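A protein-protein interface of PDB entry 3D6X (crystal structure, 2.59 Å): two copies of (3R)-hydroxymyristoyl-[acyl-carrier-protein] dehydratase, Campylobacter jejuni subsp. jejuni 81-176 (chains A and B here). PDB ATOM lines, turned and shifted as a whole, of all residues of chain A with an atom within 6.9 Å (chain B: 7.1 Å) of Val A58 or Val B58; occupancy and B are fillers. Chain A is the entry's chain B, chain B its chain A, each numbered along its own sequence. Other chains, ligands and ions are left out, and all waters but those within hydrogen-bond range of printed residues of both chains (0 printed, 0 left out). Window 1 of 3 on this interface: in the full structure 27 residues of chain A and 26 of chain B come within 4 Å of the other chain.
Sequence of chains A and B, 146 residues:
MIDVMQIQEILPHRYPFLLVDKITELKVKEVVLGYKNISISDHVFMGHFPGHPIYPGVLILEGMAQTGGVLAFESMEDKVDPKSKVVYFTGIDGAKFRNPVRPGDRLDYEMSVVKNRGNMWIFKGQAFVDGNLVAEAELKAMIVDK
Phe A17 touches Pro B56, and with the chains exchanged Pro A56 touches Phe B17.
Val A58 touches Phe B17, but with the chains exchanged Phe A17 does not touch Val B58 (4.1 Å).
Val A58 touches its own counterpart, Val B58.
Val A58 touches Glu B62, and with the chains exchanged Glu A62 touches Val B58.
14 positions are printed for both chains.
Of the printed residues of chain A, Val B58 touches Val A58 and Glu A62.
No residue of chain B comes within 4 Å of Gly A57.
Of the printed residues of chain A, Pro B56 touches Phe A17 (3.4 Å).
Of the printed residues of chain A, Glu B62 touches Val A58 (3.9 Å).
Leu B19 touches none of the printed residues of chain A.
Ile A60 touches none of the printed residues of chain B.
The nearest printed residue of chain A that does not touch Phe B17 is Leu A59 (4.2 Å).
Among the printed residues, merely in contact across the chains: Phe A17 with Pro B56, Pro A56 with Phe B17, Val A58 with Val B58, Glu A62 with Val B58, Val A58 with Glu B62 and Val A58 with Phe B17.
Printed residues of chain A that touch a printed residue of chain B: Phe A17, Pro A56, Val A58 and Glu A62.
Hydrophobic or aromatic side chains of chain B that line the printed part of chain A: Phe B17, Pro B56 and Val B58.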
ATOM      1  N   PHE A  17     -18.370  25.982  -6.416  1.00  0.00           N
ATOM      2  CA  PHE A  17     -18.292  24.804  -5.574  1.00  0.00           C
ATOM      3  C   PHE A  17     -16.845  24.301  -5.444  1.00  0.00           C
ATOM      4  O   PHE A  17     -16.589  23.109  -5.306  1.00  0.00           O
ATOM      5  CB  PHE A  17     -19.260  23.724  -6.111  1.00  0.00           C
ATOM      6  CG  PHE A  17     -19.948  22.940  -5.037  1.00  0.00           C
ATOM      7  CD1 PHE A  17     -19.550  21.650  -4.735  1.00  0.00           C
ATOM      8  CD2 PHE A  17     -20.987  23.492  -4.321  1.00  0.00           C
ATOM      9  CE1 PHE A  17     -20.198  20.904  -3.716  1.00  0.00           C
ATOM     10  CE2 PHE A  17     -21.646  22.765  -3.296  1.00  0.00           C
ATOM     11  CZ  PHE A  17     -21.249  21.470  -2.998  1.00  0.00           C
ATOM     12  N   LEU A  19     -14.117  24.392  -2.892  1.00  0.00           N
ATOM     13  CA  LEU A  19     -14.026  24.721  -1.457  1.00  0.00           C
ATOM     14  C   LEU A  19     -12.650  24.521  -0.818  1.00  0.00           C
ATOM     15  O   LEU A  19     -12.533  24.345   0.401  1.00  0.00           O
ATOM     16  CB  LEU A  19     -15.098  23.964  -0.689  1.00  0.00           C
ATOM     17  CG  LEU A  19     -16.460  24.115  -1.383  1.00  0.00           C
ATOM     18  CD1 LEU A  19     -17.600  23.607  -0.515  1.00  0.00           C
ATOM     19  CD2 LEU A  19     -16.681  25.573  -1.729  1.00  0.00           C
ATOM     20  N   TYR A  55     -21.182  28.816   8.595  1.00  0.00           N
ATOM     21  CA  TYR A  55     -20.774  27.926   7.484  1.00  0.00           C
ATOM     22  C   TYR A  55     -21.441  26.564   7.563  1.00  0.00           C
ATOM     23  O   TYR A  55     -21.278  25.851   8.531  1.00  0.00           O
ATOM     24  CB  TYR A  55     -19.260  27.745   7.447  1.00  0.00           C
ATOM     25  CG  TYR A  55     -18.759  27.361   6.090  1.00  0.00           C
ATOM     26  CD1 TYR A  55     -18.007  26.190   5.911  1.00  0.00           C
ATOM     27  CD2 TYR A  55     -19.011  28.153   4.986  1.00  0.00           C
ATOM     28  CE1 TYR A  55     -17.536  25.820   4.678  1.00  0.00           C
ATOM     29  CE2 TYR A  55     -18.529  27.783   3.728  1.00  0.00           C
ATOM     30  CZ  TYR A  55     -17.806  26.613   3.599  1.00  0.00           C
ATOM     31  OH  TYR A  55     -17.321  26.209   2.387  1.00  0.00           O
ATOM     32  N   PRO A  56     -22.183  26.191   6.526  1.00  0.00           N
ATOM     33  CA  PRO A  56     -22.914  24.921   6.535  1.00  0.00           C
ATOM     34  C   PRO A  56     -21.994  23.699   6.755  1.00  0.00           C
ATOM     35  O   PRO A  56     -20.997  23.518   6.023  1.00  0.00           O
ATOM     36  CB  PRO A  56     -23.508  24.874   5.131  1.00  0.00           C
ATOM     37  CG  PRO A  56     -23.542  26.309   4.675  1.00  0.00           C
ATOM     38  CD  PRO A  56     -22.348  26.921   5.264  1.00  0.00           C
ATOM     39  N   GLY A  57     -22.315  22.885   7.749  1.00  0.00           N
ATOM     40  CA  GLY A  57     -21.528  21.707   8.050  1.00  0.00           C
ATOM     41  C   GLY A  57     -21.264  20.824   6.844  1.00  0.00           C
ATOM     42  O   GLY A  57     -20.121  20.397   6.600  1.00  0.00           O
ATOM     43  N   VAL A  58     -22.294  20.540   6.065  1.00  0.00           N
ATOM     44  CA  VAL A  58     -22.074  19.716   4.875  1.00  0.00           C
ATOM     45  C   VAL A  58     -20.992  20.261   3.933  1.00  0.00           C
ATOM     46  O   VAL A  58     -20.355  19.505   3.206  1.00  0.00           O
ATOM     47  CB  VAL A  58     -23.364  19.485   4.036  1.00  0.00           C
ATOM     48  CG1 VAL A  58     -24.352  18.673   4.811  1.00  0.00           C
ATOM     49  CG2 VAL A  58     -23.987  20.799   3.567  1.00  0.00           C
ATOM     50  N   LEU A  59     -20.776  21.565   3.920  1.00  0.00           N
ATOM     51  CA  LEU A  59     -19.779  22.093   3.009  1.00  0.00           C
ATOM     52  C   LEU A  59     -18.410  21.813   3.551  1.00  0.00           C
ATOM     53  O   LEU A  59     -17.475  21.682   2.760  1.00  0.00           O
ATOM     54  CB  LEU A  59     -19.934  23.584   2.748  1.00  0.00           C
ATOM     55  CG  LEU A  59     -21.181  24.058   1.983  1.00  0.00           C
ATOM     56  CD1 LEU A  59     -21.213  25.625   1.742  1.00  0.00           C
ATOM     57  CD2 LEU A  59     -21.477  23.237   0.669  1.00  0.00           C
ATOM     58  N   ILE A  60     -18.273  21.728   4.878  1.00  0.00           N
ATOM     59  CA  ILE A  60     -16.995  21.378   5.453  1.00  0.00           C
ATOM     60  C   ILE A  60     -16.651  19.958   5.015  1.00  0.00           C
ATOM     61  O   ILE A  60     -15.536  19.696   4.615  1.00  0.00           O
ATOM     62  CB  ILE A  60     -17.031  21.464   6.952  1.00  0.00           C
ATOM     63  CG1 ILE A  60     -17.425  22.874   7.386  1.00  0.00           C
ATOM     64  CG2 ILE A  60     -15.669  21.144   7.505  1.00  0.00           C
ATOM     65  CD1 ILE A  60     -17.783  23.036   8.882  1.00  0.00           C
ATOM     66  N   LEU A  61     -17.616  19.038   5.058  1.00  0.00           N
ATOM     67  CA  LEU A  61     -17.402  17.685   4.504  1.00  0.00           C
ATOM     68  C   LEU A  61     -16.912  17.742   3.069  1.00  0.00           C
ATOM     69  O   LEU A  61     -15.957  17.040   2.717  1.00  0.00           O
ATOM     70  CB  LEU A  61     -18.665  16.825   4.556  1.00  0.00           C
ATOM     71  CG  LEU A  61     -19.157  16.490   5.964  1.00  0.00           C
ATOM     72  CD1 LEU A  61     -20.467  15.678   6.017  1.00  0.00           C
ATOM     73  CD2 LEU A  61     -18.049  15.762   6.680  1.00  0.00           C
ATOM     74  N   GLU A  62     -17.547  18.557   2.232  1.00  0.00           N
ATOM     75  CA  GLU A  62     -17.152  18.581   0.823  1.00  0.00           C
ATOM     76  C   GLU A  62     -15.723  19.142   0.639  1.00  0.00           C
ATOM     77  O   GLU A  62     -14.977  18.729  -0.271  1.00  0.00           O
ATOM     78  CB  GLU A  62     -18.175  19.326  -0.032  1.00  0.00           C
ATOM     79  CG  GLU A  62     -17.721  19.669  -1.440  1.00  0.00           C
ATOM     80  CD  GLU A  62     -17.655  18.462  -2.400  1.00  0.00           C
ATOM     81  OE1 GLU A  62     -18.144  17.326  -2.101  1.00  0.00           O
ATOM     82  OE2 GLU A  62     -17.087  18.661  -3.495  1.00  0.00           O
ATOM     83  N   GLY A  63     -15.320  20.061   1.506  1.00  0.00           N
ATOM     84  CA  GLY A  63     -13.975  20.620   1.395  1.00  0.00           C
ATOM     85  C   GLY A  63     -12.967  19.553   1.780  1.00  0.00           C
ATOM     86  O   GLY A  63     -11.895  19.423   1.164  1.00  0.00           O
ATOM     87  N   ALA A  65     -13.457  16.461   1.362  1.00  0.00           N
ATOM     88  CA  ALA A  65     -13.507  15.540   0.255  1.00  0.00           C
ATOM     89  C   ALA A  65     -12.654  16.034  -0.887  1.00  0.00           C
ATOM     90  O   ALA A  65     -11.937  15.242  -1.506  1.00  0.00           O
ATOM     91  CB  ALA A  65     -14.893  15.398  -0.198  1.00  0.00           C
ATOM     92  N   ILE A  92     -19.688   8.343   3.563  1.00  0.00           N
ATOM     93  CA  ILE A  92     -19.224   9.144   4.668  1.00  0.00           C
ATOM     94  C   ILE A  92     -19.740   8.526   5.943  1.00  0.00           C
ATOM     95  O   ILE A  92     -20.893   8.098   6.007  1.00  0.00           O
ATOM     96  CB  ILE A  92     -19.724  10.548   4.554  1.00  0.00           C
ATOM     97  CG1 ILE A  92     -19.071  11.230   3.350  1.00  0.00           C
ATOM     98  CG2 ILE A  92     -19.393  11.293   5.818  1.00  0.00           C
ATOM     99  CD1 ILE A  92     -19.786  12.405   2.908  1.00  0.00           C
ATOM    100  N   PHE A  97     -20.181  17.196  13.839  1.00  0.00           N
ATOM    101  CA  PHE A  97     -19.951  18.632  13.833  1.00  0.00           C
ATOM    102  C   PHE A  97     -19.854  19.153  15.239  1.00  0.00           C
ATOM    103  O   PHE A  97     -20.728  18.908  16.048  1.00  0.00           O
ATOM    104  CB  PHE A  97     -21.056  19.349  13.071  1.00  0.00           C
ATOM    105  CG  PHE A  97     -21.223  18.845  11.685  1.00  0.00           C
ATOM    106  CD1 PHE A  97     -22.324  18.091  11.337  1.00  0.00           C
ATOM    107  CD2 PHE A  97     -20.246  19.062  10.746  1.00  0.00           C
ATOM    108  CE1 PHE A  97     -22.465  17.602  10.069  1.00  0.00           C
ATOM    109  CE2 PHE A  97     -20.379  18.569   9.459  1.00  0.00           C
ATOM    110  CZ  PHE A  97     -21.483  17.842   9.127  1.00  0.00           C
ATOM    111  N   PHE B  17     -29.461  28.695   0.201  1.00  0.00           N
ATOM    112  CA  PHE B  17     -29.237  27.445   0.885  1.00  0.00           C
ATOM    113  C   PHE B  17     -30.546  26.838   1.431  1.00  0.00           C
ATOM    114  O   PHE B  17     -30.550  26.231   2.495  1.00  0.00           O
ATOM    115  CB  PHE B  17     -28.143  27.618   1.956  1.00  0.00           C
ATOM    116  CG  PHE B  17     -27.223  26.427   2.083  1.00  0.00           C
ATOM    117  CD1 PHE B  17     -27.382  25.503   3.110  1.00  0.00           C
ATOM    118  CD2 PHE B  17     -26.197  26.214   1.155  1.00  0.00           C
ATOM    119  CE1 PHE B  17     -26.544  24.412   3.218  1.00  0.00           C
ATOM    120  CE2 PHE B  17     -25.341  25.098   1.254  1.00  0.00           C
ATOM    121  CZ  PHE B  17     -25.524  24.210   2.283  1.00  0.00           C
ATOM    122  N   LEU B  19     -33.000  24.047   0.466  1.00  0.00           N
ATOM    123  CA  LEU B  19     -32.926  22.909  -0.467  1.00  0.00           C
ATOM    124  C   LEU B  19     -34.132  21.979  -0.405  1.00  0.00           C
ATOM    125  O   LEU B  19     -34.035  20.777  -0.754  1.00  0.00           O
ATOM    126  CB  LEU B  19     -31.621  22.134  -0.255  1.00  0.00           C
ATOM    127  CG  LEU B  19     -30.354  23.009  -0.198  1.00  0.00           C
ATOM    128  CD1 LEU B  19     -29.142  22.166   0.096  1.00  0.00           C
ATOM    129  CD2 LEU B  19     -30.133  23.783  -1.473  1.00  0.00           C
ATOM    130  N   TYR B  55     -25.485  17.007  -9.363  1.00  0.00           N
ATOM    131  CA  TYR B  55     -25.882  17.604  -8.081  1.00  0.00           C
ATOM    132  C   TYR B  55     -24.960  17.109  -6.946  1.00  0.00           C
ATOM    133  O   TYR B  55     -24.815  15.908  -6.718  1.00  0.00           O
ATOM    134  CB  TYR B  55     -27.340  17.271  -7.790  1.00  0.00           C
ATOM    135  CG  TYR B  55     -27.928  18.181  -6.797  1.00  0.00           C
ATOM    136  CD1 TYR B  55     -28.486  17.690  -5.623  1.00  0.00           C
ATOM    137  CD2 TYR B  55     -27.890  19.538  -6.998  1.00  0.00           C
ATOM    138  CE1 TYR B  55     -29.004  18.526  -4.683  1.00  0.00           C
ATOM    139  CE2 TYR B  55     -28.424  20.406  -6.067  1.00  0.00           C
ATOM    140  CZ  TYR B  55     -28.983  19.888  -4.909  1.00  0.00           C
ATOM    141  OH  TYR B  55     -29.518  20.750  -3.973  1.00  0.00           O
ATOM    142  N   PRO B  56     -24.308  18.032  -6.253  1.00  0.00           N
ATOM    143  CA  PRO B  56     -23.370  17.583  -5.216  1.00  0.00           C
ATOM    144  C   PRO B  56     -24.013  16.680  -4.152  1.00  0.00           C
ATOM    145  O   PRO B  56     -25.016  17.054  -3.540  1.00  0.00           O
ATOM    146  CB  PRO B  56     -22.897  18.898  -4.597  1.00  0.00           C
ATOM    147  CG  PRO B  56     -23.033  19.919  -5.737  1.00  0.00           C
ATOM    148  CD  PRO B  56     -24.346  19.495  -6.387  1.00  0.00           C
ATOM    149  N   GLY B  57     -23.432  15.502  -3.929  1.00  0.00           N
ATOM    150  CA  GLY B  57     -23.883  14.601  -2.858  1.00  0.00           C
ATOM    151  C   GLY B  57     -24.135  15.269  -1.521  1.00  0.00           C
ATOM    152  O   GLY B  57     -25.181  15.102  -0.919  1.00  0.00           O
ATOM    153  N   VAL B  58     -23.192  16.058  -1.041  1.00  0.00           N
ATOM    154  CA  VAL B  58     -23.400  16.652   0.277  1.00  0.00           C
ATOM    155  C   VAL B  58     -24.642  17.524   0.326  1.00  0.00           C
ATOM    156  O   VAL B  58     -25.233  17.655   1.385  1.00  0.00           O
ATOM    157  CB  VAL B  58     -22.200  17.462   0.815  1.00  0.00           C
ATOM    158  CG1 VAL B  58     -20.973  16.626   0.810  1.00  0.00           C
ATOM    159  CG2 VAL B  58     -22.021  18.761   0.023  1.00  0.00           C
ATOM    160  N   LEU B  59     -25.046  18.124  -0.794  1.00  0.00           N
ATOM    161  CA  LEU B  59     -26.273  18.905  -0.756  1.00  0.00           C
ATOM    162  C   LEU B  59     -27.515  18.002  -0.632  1.00  0.00           C
ATOM    163  O   LEU B  59     -28.559  18.448  -0.085  1.00  0.00           O
ATOM    164  CB  LEU B  59     -26.399  19.883  -1.927  1.00  0.00           C
ATOM    165  CG  LEU B  59     -25.332  20.987  -2.051  1.00  0.00           C
ATOM    166  CD1 LEU B  59     -25.695  21.989  -3.084  1.00  0.00           C
ATOM    167  CD2 LEU B  59     -25.074  21.682  -0.734  1.00  0.00           C
ATOM    168  N   ILE B  60     -27.440  16.756  -1.123  1.00  0.00           N
ATOM    169  CA  ILE B  60     -28.564  15.877  -0.919  1.00  0.00           C
ATOM    170  C   ILE B  60     -28.741  15.644   0.577  1.00  0.00           C
ATOM    171  O   ILE B  60     -29.843  15.734   1.080  1.00  0.00           O
ATOM    172  CB  ILE B  60     -28.420  14.547  -1.652  1.00  0.00           C
ATOM    173  CG1 ILE B  60     -28.214  14.792  -3.151  1.00  0.00           C
ATOM    174  CG2 ILE B  60     -29.681  13.684  -1.450  1.00  0.00           C
ATOM    175  CD1 ILE B  60     -27.865  13.522  -3.980  1.00  0.00           C
ATOM    176  N   LEU B  61     -27.652  15.370   1.289  1.00  0.00           N
ATOM    177  CA  LEU B  61     -27.724  15.221   2.741  1.00  0.00           C
ATOM    178  C   LEU B  61     -28.320  16.466   3.404  1.00  0.00           C
ATOM    179  O   LEU B  61     -29.110  16.346   4.330  1.00  0.00           O
ATOM    180  CB  LEU B  61     -26.347  14.959   3.348  1.00  0.00           C
ATOM    181  CG  LEU B  61     -25.497  13.755   2.919  1.00  0.00           C
ATOM    182  CD1 LEU B  61     -24.042  13.903   3.400  1.00  0.00           C
ATOM    183  CD2 LEU B  61     -26.082  12.446   3.393  1.00  0.00           C
ATOM    184  N   GLU B  62     -27.931  17.655   2.959  1.00  0.00           N
ATOM    185  CA  GLU B  62     -28.454  18.868   3.575  1.00  0.00           C
ATOM    186  C   GLU B  62     -29.957  18.978   3.380  1.00  0.00           C
ATOM    187  O   GLU B  62     -30.673  19.459   4.273  1.00  0.00           O
ATOM    188  CB  GLU B  62     -27.798  20.083   2.951  1.00  0.00           C
ATOM    189  CG  GLU B  62     -28.381  21.414   3.392  1.00  0.00           C
ATOM    190  CD  GLU B  62     -28.159  21.723   4.865  1.00  0.00           C
ATOM    191  OE1 GLU B  62     -27.385  21.020   5.538  1.00  0.00           O
ATOM    192  OE2 GLU B  62     -28.762  22.691   5.355  1.00  0.00           O
ATOM    193  N   GLY B  63     -30.429  18.551   2.196  1.00  0.00           N
ATOM    194  CA  GLY B  63     -31.853  18.564   1.865  1.00  0.00           C
ATOM    195  C   GLY B  63     -32.601  17.617   2.792  1.00  0.00           C
ATOM    196  O   GLY B  63     -33.662  17.966   3.348  1.00  0.00           O
ATOM    197  N   ALA B  65     -31.603  16.779   5.696  1.00  0.00           N
ATOM    198  CA  ALA B  65     -31.547  17.362   7.026  1.00  0.00           C
ATOM    199  C   ALA B  65     -32.612  18.440   7.190  1.00  0.00           C
ATOM    200  O   ALA B  65     -33.207  18.592   8.252  1.00  0.00           O
ATOM    201  CB  ALA B  65     -30.164  17.923   7.302  1.00  0.00           C
ATOM    202  N   ILE B  92     -23.793  12.665  11.087  1.00  0.00           N
ATOM    203  CA  ILE B  92     -24.278  11.888   9.960  1.00  0.00           C
ATOM    204  C   ILE B  92     -23.472  10.616   9.903  1.00  0.00           C
ATOM    205  O   ILE B  92     -22.247  10.634  10.082  1.00  0.00           O
ATOM    206  CB  ILE B  92     -24.120  12.608   8.602  1.00  0.00           C
ATOM    207  CG1 ILE B  92     -24.846  13.949   8.594  1.00  0.00           C
ATOM    208  CG2 ILE B  92     -24.657  11.734   7.465  1.00  0.00           C
ATOM    209  CD1 ILE B  92     -24.513  14.796   7.398  1.00  0.00           C
ATOM    210  N   PHE B  97     -23.699   7.332  -1.323  1.00  0.00           N
ATOM    211  CA  PHE B  97     -24.231   7.867  -2.571  1.00  0.00           C
ATOM    212  C   PHE B  97     -24.217   6.814  -3.665  1.00  0.00           C
ATOM    213  O   PHE B  97     -23.204   6.155  -3.920  1.00  0.00           O
ATOM    214  CB  PHE B  97     -23.449   9.082  -3.027  1.00  0.00           C
ATOM    215  CG  PHE B  97     -23.208  10.035  -1.941  1.00  0.00           C
ATOM    216  CD1 PHE B  97     -21.990  10.092  -1.322  1.00  0.00           C
ATOM    217  CD2 PHE B  97     -24.222  10.835  -1.495  1.00  0.00           C
ATOM    218  CE1 PHE B  97     -21.789  10.948  -0.278  1.00  0.00           C
ATOM    219  CE2 PHE B  97     -24.026  11.683  -0.470  1.00  0.00           C
ATOM    220  CZ  PHE B  97     -22.813  11.738   0.148  1.00  0.00           C
